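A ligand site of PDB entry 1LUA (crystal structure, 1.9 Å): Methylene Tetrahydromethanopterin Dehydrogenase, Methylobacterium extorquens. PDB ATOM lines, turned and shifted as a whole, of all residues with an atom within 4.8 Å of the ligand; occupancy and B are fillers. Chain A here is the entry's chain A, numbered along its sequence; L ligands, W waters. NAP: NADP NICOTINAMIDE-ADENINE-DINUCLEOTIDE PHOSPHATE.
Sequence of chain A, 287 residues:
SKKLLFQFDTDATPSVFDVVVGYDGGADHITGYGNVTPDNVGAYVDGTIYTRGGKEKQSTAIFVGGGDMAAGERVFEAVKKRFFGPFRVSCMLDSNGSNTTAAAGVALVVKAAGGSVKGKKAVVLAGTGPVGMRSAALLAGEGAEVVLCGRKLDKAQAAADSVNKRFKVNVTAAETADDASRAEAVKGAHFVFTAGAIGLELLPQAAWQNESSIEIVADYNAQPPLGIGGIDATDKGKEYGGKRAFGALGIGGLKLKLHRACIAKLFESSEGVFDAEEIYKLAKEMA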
ATOM      1  N   PHE A  17       9.071 -21.077  -7.820  1.00  0.00           N
ATOM      2  CA  PHE A  17      10.179 -20.272  -7.305  1.00  0.00           C
ATOM      3  C   PHE A  17       9.789 -18.783  -7.352  1.00  0.00           C
ATOM      4  O   PHE A  17       9.973 -18.057  -6.378  1.00  0.00           O
ATOM      5  CB  PHE A  17      11.444 -20.533  -8.174  1.00  0.00           C
ATOM      6  CG  PHE A  17      12.707 -19.869  -7.674  1.00  0.00           C
ATOM      7  CD1 PHE A  17      13.723 -20.624  -7.101  1.00  0.00           C
ATOM      8  CD2 PHE A  17      12.868 -18.483  -7.766  1.00  0.00           C
ATOM      9  CE1 PHE A  17      14.901 -20.007  -6.636  1.00  0.00           C
ATOM     10  CE2 PHE A  17      14.046 -17.866  -7.301  1.00  0.00           C
ATOM     11  CZ  PHE A  17      15.061 -18.633  -6.735  1.00  0.00           C
ATOM     12  N   ASN A  96      13.446 -17.236 -15.647  1.00  0.00           N
ATOM     13  CA  ASN A  96      14.411 -18.177 -15.061  1.00  0.00           C
ATOM     14  C   ASN A  96      15.445 -17.507 -14.162  1.00  0.00           C
ATOM     15  O   ASN A  96      16.493 -18.086 -13.905  1.00  0.00           O
ATOM     16  CB  ASN A  96      15.115 -18.962 -16.170  1.00  0.00           C
ATOM     17  CG  ASN A  96      15.447 -20.386 -15.770  1.00  0.00           C
ATOM     18  OD1 ASN A  96      14.604 -21.108 -15.234  1.00  0.00           O
ATOM     19  ND2 ASN A  96      16.673 -20.805 -16.023  1.00  0.00           N
ATOM     20  N   GLY A  97      15.159 -16.286 -13.724  1.00  0.00           N
ATOM     21  CA  GLY A  97      16.079 -15.578 -12.848  1.00  0.00           C
ATOM     22  C   GLY A  97      17.378 -15.139 -13.526  1.00  0.00           C
ATOM     23  O   GLY A  97      18.361 -14.842 -12.839  1.00  0.00           O
ATOM     24  N   SER A  98      17.382 -15.051 -14.850  1.00  0.00           N
ATOM     25  CA  SER A  98      18.621 -14.667 -15.538  1.00  0.00           C
ATOM     26  C   SER A  98      19.063 -13.229 -15.379  1.00  0.00           C
ATOM     27  O   SER A  98      20.283 -12.955 -15.317  1.00  0.00           O
ATOM     28  CB  SER A  98      18.537 -15.011 -17.016  1.00  0.00           C
ATOM     29  OG  SER A  98      18.440 -16.412 -17.177  1.00  0.00           O
ATOM     30  N   THR A 101      20.285 -12.926 -11.628  1.00  0.00           N
ATOM     31  CA  THR A 101      21.525 -13.668 -11.397  1.00  0.00           C
ATOM     32  C   THR A 101      22.671 -12.933 -12.110  1.00  0.00           C
ATOM     33  O   THR A 101      23.702 -12.669 -11.503  1.00  0.00           O
ATOM     34  CB  THR A 101      21.395 -15.124 -11.901  1.00  0.00           C
ATOM     35  OG1 THR A 101      20.428 -15.816 -11.102  1.00  0.00           O
ATOM     36  CG2 THR A 101      22.758 -15.859 -11.809  1.00  0.00           C
ATOM     37  N   ALA A 126      31.229 -20.253 -22.099  1.00  0.00           N
ATOM     38  CA  ALA A 126      29.902 -20.834 -22.262  1.00  0.00           C
ATOM     39  C   ALA A 126      28.917 -19.682 -22.096  1.00  0.00           C
ATOM     40  O   ALA A 126      27.885 -19.821 -21.447  1.00  0.00           O
ATOM     41  CB  ALA A 126      29.657 -21.901 -21.205  1.00  0.00           C
ATOM     42  N   THR A 128      26.842 -18.334 -24.154  1.00  0.00           N
ATOM     43  CA  THR A 128      25.724 -18.356 -25.110  1.00  0.00           C
ATOM     44  C   THR A 128      24.337 -18.525 -24.514  1.00  0.00           C
ATOM     45  O   THR A 128      23.337 -18.435 -25.232  1.00  0.00           O
ATOM     46  CB  THR A 128      25.921 -19.461 -26.172  1.00  0.00           C
ATOM     47  OG1 THR A 128      26.184 -20.725 -25.533  1.00  0.00           O
ATOM     48  CG2 THR A 128      27.075 -19.105 -27.079  1.00  0.00           C
ATOM     49  N   GLY A 129      24.265 -18.810 -23.218  1.00  0.00           N
ATOM     50  CA  GLY A 129      22.973 -18.955 -22.548  1.00  0.00           C
ATOM     51  C   GLY A 129      22.497 -17.591 -22.046  1.00  0.00           C
ATOM     52  O   GLY A 129      23.245 -16.619 -22.133  1.00  0.00           O
ATOM     53  N   PRO A 130      21.265 -17.482 -21.516  1.00  0.00           N
ATOM     54  CA  PRO A 130      20.744 -16.207 -21.021  1.00  0.00           C
ATOM     55  C   PRO A 130      21.591 -15.513 -19.925  1.00  0.00           C
ATOM     56  O   PRO A 130      21.732 -14.312 -19.939  1.00  0.00           O
ATOM     57  CB  PRO A 130      19.321 -16.572 -20.535  1.00  0.00           C
ATOM     58  CG  PRO A 130      19.407 -18.004 -20.217  1.00  0.00           C
ATOM     59  CD  PRO A 130      20.303 -18.582 -21.291  1.00  0.00           C
ATOM     60  N   VAL A 131      22.125 -16.269 -18.972  1.00  0.00           N
ATOM     61  CA  VAL A 131      22.939 -15.639 -17.932  1.00  0.00           C
ATOM     62  C   VAL A 131      24.258 -15.108 -18.502  1.00  0.00           C
ATOM     63  O   VAL A 131      24.702 -14.012 -18.171  1.00  0.00           O
ATOM     64  CB  VAL A 131      23.203 -16.629 -16.771  1.00  0.00           C
ATOM     65  CG1 VAL A 131      24.194 -16.031 -15.789  1.00  0.00           C
ATOM     66  CG2 VAL A 131      21.900 -16.924 -16.043  1.00  0.00           C
ATOM     67  N   GLY A 132      24.860 -15.891 -19.389  1.00  0.00           N
ATOM     68  CA  GLY A 132      26.117 -15.454 -19.997  1.00  0.00           C
ATOM     69  C   GLY A 132      25.913 -14.236 -20.890  1.00  0.00           C
ATOM     70  O   GLY A 132      26.712 -13.304 -20.864  1.00  0.00           O
ATOM     71  N   GLY A 150      32.039 -20.055 -26.822  1.00  0.00           N
ATOM     72  CA  GLY A 150      31.179 -21.207 -26.877  1.00  0.00           C
ATOM     73  C   GLY A 150      31.880 -22.246 -27.736  1.00  0.00           C
ATOM     74  O   GLY A 150      32.841 -21.911 -28.454  1.00  0.00           O
ATOM     75  N   ARG A 151      31.409 -23.482 -27.667  1.00  0.00           N
ATOM     76  CA  ARG A 151      32.013 -24.552 -28.452  1.00  0.00           C
ATOM     77  C   ARG A 151      31.997 -24.304 -29.965  1.00  0.00           C
ATOM     78  O   ARG A 151      32.958 -24.655 -30.664  1.00  0.00           O
ATOM     79  CB  ARG A 151      31.319 -25.867 -28.124  1.00  0.00           C
ATOM     80  CG  ARG A 151      31.615 -26.373 -26.714  1.00  0.00           C
ATOM     81  CD  ARG A 151      30.677 -27.489 -26.313  1.00  0.00           C
ATOM     82  NE  ARG A 151      29.304 -27.019 -26.269  1.00  0.00           N
ATOM     83  CZ  ARG A 151      28.252 -27.779 -25.961  1.00  0.00           C
ATOM     84  NH1 ARG A 151      28.428 -29.057 -25.673  1.00  0.00           N
ATOM     85  NH2 ARG A 151      27.032 -27.259 -25.929  1.00  0.00           N
ATOM     86  N   LYS A 155      27.126 -20.154 -33.124  1.00  0.00           N
ATOM     87  CA  LYS A 155      26.231 -19.910 -31.996  1.00  0.00           C
ATOM     88  C   LYS A 155      26.799 -18.795 -31.133  1.00  0.00           C
ATOM     89  O   LYS A 155      26.057 -17.941 -30.628  1.00  0.00           O
ATOM     90  CB  LYS A 155      26.087 -21.185 -31.169  1.00  0.00           C
ATOM     91  CG  LYS A 155      25.175 -21.104 -29.958  1.00  0.00           C
ATOM     92  CD  LYS A 155      25.062 -22.498 -29.333  1.00  0.00           C
ATOM     93  CE  LYS A 155      24.094 -22.530 -28.144  1.00  0.00           C
ATOM     94  NZ  LYS A 155      23.993 -23.890 -27.570  1.00  0.00           N
ATOM     95  N   ARG A 182      39.756 -23.177 -24.214  1.00  0.00           N
ATOM     96  CA  ARG A 182      39.245 -22.351 -23.122  1.00  0.00           C
ATOM     97  C   ARG A 182      40.366 -21.756 -22.276  1.00  0.00           C
ATOM     98  O   ARG A 182      40.240 -20.665 -21.740  1.00  0.00           O
ATOM     99  CB  ARG A 182      38.280 -23.145 -22.237  1.00  0.00           C
ATOM    100  CG  ARG A 182      36.937 -23.442 -22.914  1.00  0.00           C
ATOM    101  CD  ARG A 182      35.826 -23.702 -21.907  1.00  0.00           C
ATOM    102  NE  ARG A 182      35.909 -25.005 -21.272  1.00  0.00           N
ATOM    103  CZ  ARG A 182      35.478 -26.135 -21.813  1.00  0.00           C
ATOM    104  NH1 ARG A 182      34.932 -26.138 -23.030  1.00  0.00           N
ATOM    105  NH2 ARG A 182      35.571 -27.281 -21.143  1.00  0.00           N
ATOM    106  N   ALA A 195      29.695 -19.257 -17.285  1.00  0.00           N
ATOM    107  CA  ALA A 195      28.238 -19.279 -17.270  1.00  0.00           C
ATOM    108  C   ALA A 195      27.719 -20.555 -17.930  1.00  0.00           C
ATOM    109  O   ALA A 195      26.748 -20.516 -18.692  1.00  0.00           O
ATOM    110  CB  ALA A 195      27.676 -18.061 -18.014  1.00  0.00           C
ATOM    111  N   GLY A 196      28.378 -21.668 -17.621  1.00  0.00           N
ATOM    112  CA  GLY A 196      27.962 -22.930 -18.202  1.00  0.00           C
ATOM    113  C   GLY A 196      26.732 -23.585 -17.595  1.00  0.00           C
ATOM    114  O   GLY A 196      26.289 -23.231 -16.505  1.00  0.00           O
ATOM    115  N   ALA A 197      26.172 -24.535 -18.331  1.00  0.00           N
ATOM    116  CA  ALA A 197      24.993 -25.273 -17.894  1.00  0.00           C
ATOM    117  C   ALA A 197      25.315 -25.947 -16.565  1.00  0.00           C
ATOM    118  O   ALA A 197      26.473 -26.124 -16.206  1.00  0.00           O
ATOM    119  CB  ALA A 197      24.607 -26.295 -18.929  1.00  0.00           C
ATOM    120  N   ILE A 198      24.265 -26.329 -15.851  1.00  0.00           N
ATOM    121  CA  ILE A 198      24.427 -26.932 -14.537  1.00  0.00           C
ATOM    122  C   ILE A 198      25.221 -28.241 -14.470  1.00  0.00           C
ATOM    123  O   ILE A 198      25.015 -29.158 -15.280  1.00  0.00           O
ATOM    124  CB  ILE A 198      23.038 -27.129 -13.891  1.00  0.00           C
ATOM    125  CG1 ILE A 198      23.203 -27.678 -12.468  1.00  0.00           C
ATOM    126  CG2 ILE A 198      22.193 -28.060 -14.753  1.00  0.00           C
ATOM    127  CD1 ILE A 198      21.885 -27.841 -11.700  1.00  0.00           C
ATOM    128  N   LEU A 200      28.735 -28.787 -14.786  1.00  0.00           N
ATOM    129  CA  LEU A 200      29.860 -28.954 -15.718  1.00  0.00           C
ATOM    130  C   LEU A 200      31.042 -28.066 -15.339  1.00  0.00           C
ATOM    131  O   LEU A 200      30.842 -26.946 -14.830  1.00  0.00           O
ATOM    132  CB  LEU A 200      29.432 -28.584 -17.138  1.00  0.00           C
ATOM    133  CG  LEU A 200      28.849 -29.587 -18.133  1.00  0.00           C
ATOM    134  CD1 LEU A 200      28.260 -30.821 -17.433  1.00  0.00           C
ATOM    135  CD2 LEU A 200      27.801 -28.859 -18.954  1.00  0.00           C
ATOM    136  N   LEU A 202      34.507 -25.936 -16.515  1.00  0.00           N
ATOM    137  CA  LEU A 202      34.987 -25.243 -17.706  1.00  0.00           C
ATOM    138  C   LEU A 202      36.395 -24.702 -17.586  1.00  0.00           C
ATOM    139  O   LEU A 202      37.081 -24.549 -18.596  1.00  0.00           O
ATOM    140  CB  LEU A 202      34.047 -24.078 -18.066  1.00  0.00           C
ATOM    141  CG  LEU A 202      32.595 -24.394 -18.420  1.00  0.00           C
ATOM    142  CD1 LEU A 202      31.820 -23.092 -18.642  1.00  0.00           C
ATOM    143  CD2 LEU A 202      32.555 -25.281 -19.658  1.00  0.00           C
ATOM    144  N   TYR A 220      28.729 -19.220 -12.135  1.00  0.00           N
ATOM    145  CA  TYR A 220      27.285 -19.250 -11.927  1.00  0.00           C
ATOM    146  C   TYR A 220      26.732 -20.648 -11.676  1.00  0.00           C
ATOM    147  O   TYR A 220      25.565 -20.793 -11.311  1.00  0.00           O
ATOM    148  CB  TYR A 220      26.550 -18.641 -13.145  1.00  0.00           C
ATOM    149  CG  TYR A 220      26.735 -17.147 -13.290  1.00  0.00           C
ATOM    150  CD1 TYR A 220      27.535 -16.602 -14.300  1.00  0.00           C
ATOM    151  CD2 TYR A 220      26.108 -16.265 -12.406  1.00  0.00           C
ATOM    152  CE1 TYR A 220      27.693 -15.208 -14.437  1.00  0.00           C
ATOM    153  CE2 TYR A 220      26.263 -14.889 -12.537  1.00  0.00           C
ATOM    154  CZ  TYR A 220      27.049 -14.361 -13.543  1.00  0.00           C
ATOM    155  OH  TYR A 220      27.132 -12.981 -13.671  1.00  0.00           O
ATOM    156  N   ASN A 221      27.556 -21.678 -11.864  1.00  0.00           N
ATOM    157  CA  ASN A 221      27.130 -23.067 -11.636  1.00  0.00           C
ATOM    158  C   ASN A 221      27.309 -23.492 -10.178  1.00  0.00           C
ATOM    159  O   ASN A 221      28.418 -23.449  -9.651  1.00  0.00           O
ATOM    160  CB  ASN A 221      27.938 -23.995 -12.553  1.00  0.00           C
ATOM    161  CG  ASN A 221      27.730 -25.471 -12.226  1.00  0.00           C
ATOM    162  OD1 ASN A 221      26.656 -25.870 -11.793  1.00  0.00           O
ATOM    163  ND2 ASN A 221      28.768 -26.281 -12.455  1.00  0.00           N
ATOM    164  N   LYS A 255      21.502 -12.377  -5.343  1.00  0.00           N
ATOM    165  CA  LYS A 255      20.418 -12.516  -6.311  1.00  0.00           C
ATOM    166  C   LYS A 255      19.071 -12.596  -5.603  1.00  0.00           C
ATOM    167  O   LYS A 255      18.095 -11.946  -6.003  1.00  0.00           O
ATOM    168  CB  LYS A 255      20.619 -13.789  -7.150  1.00  0.00           C
ATOM    169  CG  LYS A 255      19.460 -14.173  -8.067  1.00  0.00           C
ATOM    170  CD  LYS A 255      18.444 -15.066  -7.366  1.00  0.00           C
ATOM    171  CE  LYS A 255      17.210 -15.358  -8.235  1.00  0.00           C
ATOM    172  NZ  LYS A 255      17.486 -16.257  -9.408  1.00  0.00           N
HETATM  173  PA  NAP L   1      22.405 -22.819 -20.151  1.00  0.00           P
HETATM  174  O1A NAP L   1      21.781 -24.017 -19.601  1.00  0.00           O
HETATM  175  O2A NAP L   1      21.720 -22.075 -21.208  1.00  0.00           O
HETATM  176  O5B NAP L   1      23.902 -23.260 -20.615  1.00  0.00           O
HETATM  177  C5B NAP L   1      24.931 -22.290 -20.877  1.00  0.00           C
HETATM  178  C4B NAP L   1      25.842 -22.747 -21.998  1.00  0.00           C
HETATM  179  O4B NAP L   1      26.605 -23.846 -21.537  1.00  0.00           O
HETATM  180  C3B NAP L   1      25.168 -23.255 -23.244  1.00  0.00           C
HETATM  181  O3B NAP L   1      24.739 -22.174 -24.070  1.00  0.00           O
HETATM  182  C2B NAP L   1      26.297 -24.019 -23.933  1.00  0.00           C
HETATM  183  O2B NAP L   1      27.158 -23.188 -24.765  1.00  0.00           O
HETATM  184  C1B NAP L   1      27.163 -24.468 -22.733  1.00  0.00           C
HETATM  185  N9A NAP L   1      27.208 -25.935 -22.523  1.00  0.00           N
HETATM  186  C8A NAP L   1      26.191 -26.849 -22.278  1.00  0.00           C
HETATM  187  N7A NAP L   1      26.632 -28.079 -22.151  1.00  0.00           N
HETATM  188  C5A NAP L   1      28.000 -27.981 -22.325  1.00  0.00           C
HETATM  189  C6A NAP L   1      29.040 -28.949 -22.303  1.00  0.00           C
HETATM  190  N6A NAP L   1      28.796 -30.227 -22.084  1.00  0.00           N
HETATM  191  N1A NAP L   1      30.314 -28.514 -22.519  1.00  0.00           N
HETATM  192  C2A NAP L   1      30.574 -27.197 -22.739  1.00  0.00           C
HETATM  193  N3A NAP L   1      29.650 -26.224 -22.773  1.00  0.00           N
HETATM  194  C4A NAP L   1      28.370 -26.687 -22.549  1.00  0.00           C
HETATM  195  O3  NAP L   1      22.774 -21.831 -18.959  1.00  0.00           O
HETATM  196  PN  NAP L   1      22.065 -20.576 -18.233  1.00  0.00           P
HETATM  197  O1N NAP L   1      22.482 -19.356 -18.955  1.00  0.00           O
HETATM  198  O2N NAP L   1      20.606 -20.906 -18.182  1.00  0.00           O
HETATM  199  O5D NAP L   1      22.470 -20.624 -16.717  1.00  0.00           O
HETATM  200  C5D NAP L   1      23.815 -20.309 -16.330  1.00  0.00           C
HETATM  201  C4D NAP L   1      24.188 -21.000 -15.023  1.00  0.00           C
HETATM  202  O4D NAP L   1      23.711 -20.257 -13.901  1.00  0.00           O
HETATM  203  C3D NAP L   1      23.637 -22.438 -14.832  1.00  0.00           C
HETATM  204  O3D NAP L   1      24.576 -23.353 -14.246  1.00  0.00           O
HETATM  205  C2D NAP L   1      22.403 -22.282 -13.938  1.00  0.00           C
HETATM  206  O2D NAP L   1      22.210 -23.386 -13.075  1.00  0.00           O
HETATM  207  C1D NAP L   1      22.725 -20.982 -13.155  1.00  0.00           C
HETATM  208  N1N NAP L   1      21.511 -20.190 -12.852  1.00  0.00           N
HETATM  209  C2N NAP L   1      21.145 -20.205 -11.489  1.00  0.00           C
HETATM  210  C3N NAP L   1      19.971 -19.466 -11.092  1.00  0.00           C
HETATM  211  C7N NAP L   1      19.520 -19.459  -9.680  1.00  0.00           C
HETATM  212  O7N NAP L   1      18.754 -18.603  -9.220  1.00  0.00           O
HETATM  213  N7N NAP L   1      19.947 -20.391  -8.817  1.00  0.00           N
HETATM  214  C4N NAP L   1      19.262 -18.753 -12.088  1.00  0.00           C
HETATM  215  C5N NAP L   1      19.626 -18.765 -13.401  1.00  0.00           C
HETATM  216  C6N NAP L   1      20.742 -19.479 -13.790  1.00  0.00           C
HETATM  217  P2B NAP L   1      27.638 -23.548 -26.272  1.00  0.00           P
HETATM  218  O1X NAP L   1      27.707 -22.305 -27.043  1.00  0.00           O
HETATM  219  O2X NAP L   1      28.956 -24.160 -26.013  1.00  0.00           O
HETATM  220  O3X NAP L   1      26.670 -24.533 -26.759  1.00  0.00           O
HETATM  221  O   HOH W   1      21.957 -22.217 -23.807  1.00  0.00           O
HETATM  222  O   HOH W   2      19.544 -22.827 -16.197  1.00  0.00           O
HETATM  223  O   HOH W   3      24.920 -18.715 -20.177  1.00  0.00           O
HETATM  224  O   HOH W   4      18.199 -21.431 -19.407  1.00  0.00           O
HETATM  225  O   HOH W   5      23.694 -24.037 -11.039  1.00  0.00           O
HETATM  226  O   HOH W   6      21.667 -25.106 -17.156  1.00  0.00           O
HETATM  227  O   HOH W   7      28.812 -22.462 -29.361  1.00  0.00           O
HETATM  228  O   HOH W   8      23.474 -26.151 -23.921  1.00  0.00           O
HETATM  229  O   HOH W   9      30.839 -23.947 -23.881  1.00  0.00           O
HETATM  230  O   HOH W  10      21.599 -16.725  -8.579  1.00  0.00           O
HETATM  231  O   HOH W  11      18.719 -19.148 -16.646  1.00  0.00           O
HETATM  232  O   HOH W  12      19.013 -22.233 -21.839  1.00  0.00           O
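The side-chain hydroxyl (OG1) of Thr 128 is in hydrogen-bond range of an oxygen (O3B) of the ligand (2.5 Å). The side-chain amino group (NZ) of Lys 255 lies within hydrogen-bond range of an oxygen (O7N) of the ligand. The backbone carbonyl oxygen (O) of Gly 196 lies within hydrogen-bond range of an oxygen (O3D) of the ligand (2.8 Å). The side-chain amino group of Lys 155 is in salt-bridge range of an oxygen (O3X) of the ligand, 2.9 Å away. O2X of the ligand sits at hydrogen-bond distance from N of Arg 151. The guanidinium group (NH2) of Arg 151 is in salt-bridge range of an oxygen (O3X) of the ligand (2.9 Å). O1N of the ligand sits at hydrogen-bond distance from N of Val 131 (3.1 Å). O4B of the ligand is in hydrogen-bond range of N of Ala 197 (3.3 Å). O3D of the ligand sits at hydrogen-bond distance from N of Ile 198, 3.4 Å away.
The side-chain amino group of Lys 255 is in hydrogen-bond range of the side-chain hydroxyl of Thr 101, at 3.4 Å. OG1 of Thr 101 sits at hydrogen-bond distance from O of Gly 97. O of Leu 200 lies within hydrogen-bond range of ND2 of Asn 221 (3.2 Å).
An oxygen (O1N) of the ligand sits close to the backbone nitrogen of Pro 130 (3.4 Å). An oxygen (O4D) of the ligand lies close to the backbone carbonyl oxygen (O) of Tyr 220 (3.2 Å). Residues that only touch the ligand: Asn 96, Thr 101, Ala 126, Gly 129, Gly 150, Ala 195, Leu 200 and Asn 221. Hydrophobic or aromatic side chains within 4 Å of the ligand: Ala 126, Pro 130, Val 131, Ala 197, Ile 198, Leu 200 and Tyr 220. Within 4 Å of the ligand: Asn 96, Thr 101, Ala 126, Thr 128, Gly 129, Pro 130, Val 131, Gly 150, Arg 151, Lys 155, Ala 195, Gly 196, Ala 197, Ile 198, Leu 200, Tyr 220, Asn 221 and Lys 255.
Water W7 lies within hydrogen-bond range of O1X of the ligand (2.6 Å) and N of Arg 151 (3.3 Å). Water W6 lies within hydrogen-bond range of O1A of the ligand (2.7 Å) and N of Ile 198 (3.2 Å). Water W3 lies within hydrogen-bond range of an oxygen (O1N) of the ligand, the backbone NH (N) of Gly 132, the backbone carbonyl oxygen (O) of Ala 195, the backbone NH (N) of Gly 129 and the backbone carbonyl oxygen (O) of Ala 126. Water W11 lies within hydrogen-bond range of ND2 of Asn 96, OG of Ser 98 and O2N of the ligand. Water W10 lies within hydrogen-bond range of OG1 of Thr 101 (2.9 Å) and O7N of the ligand (3.5 Å).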
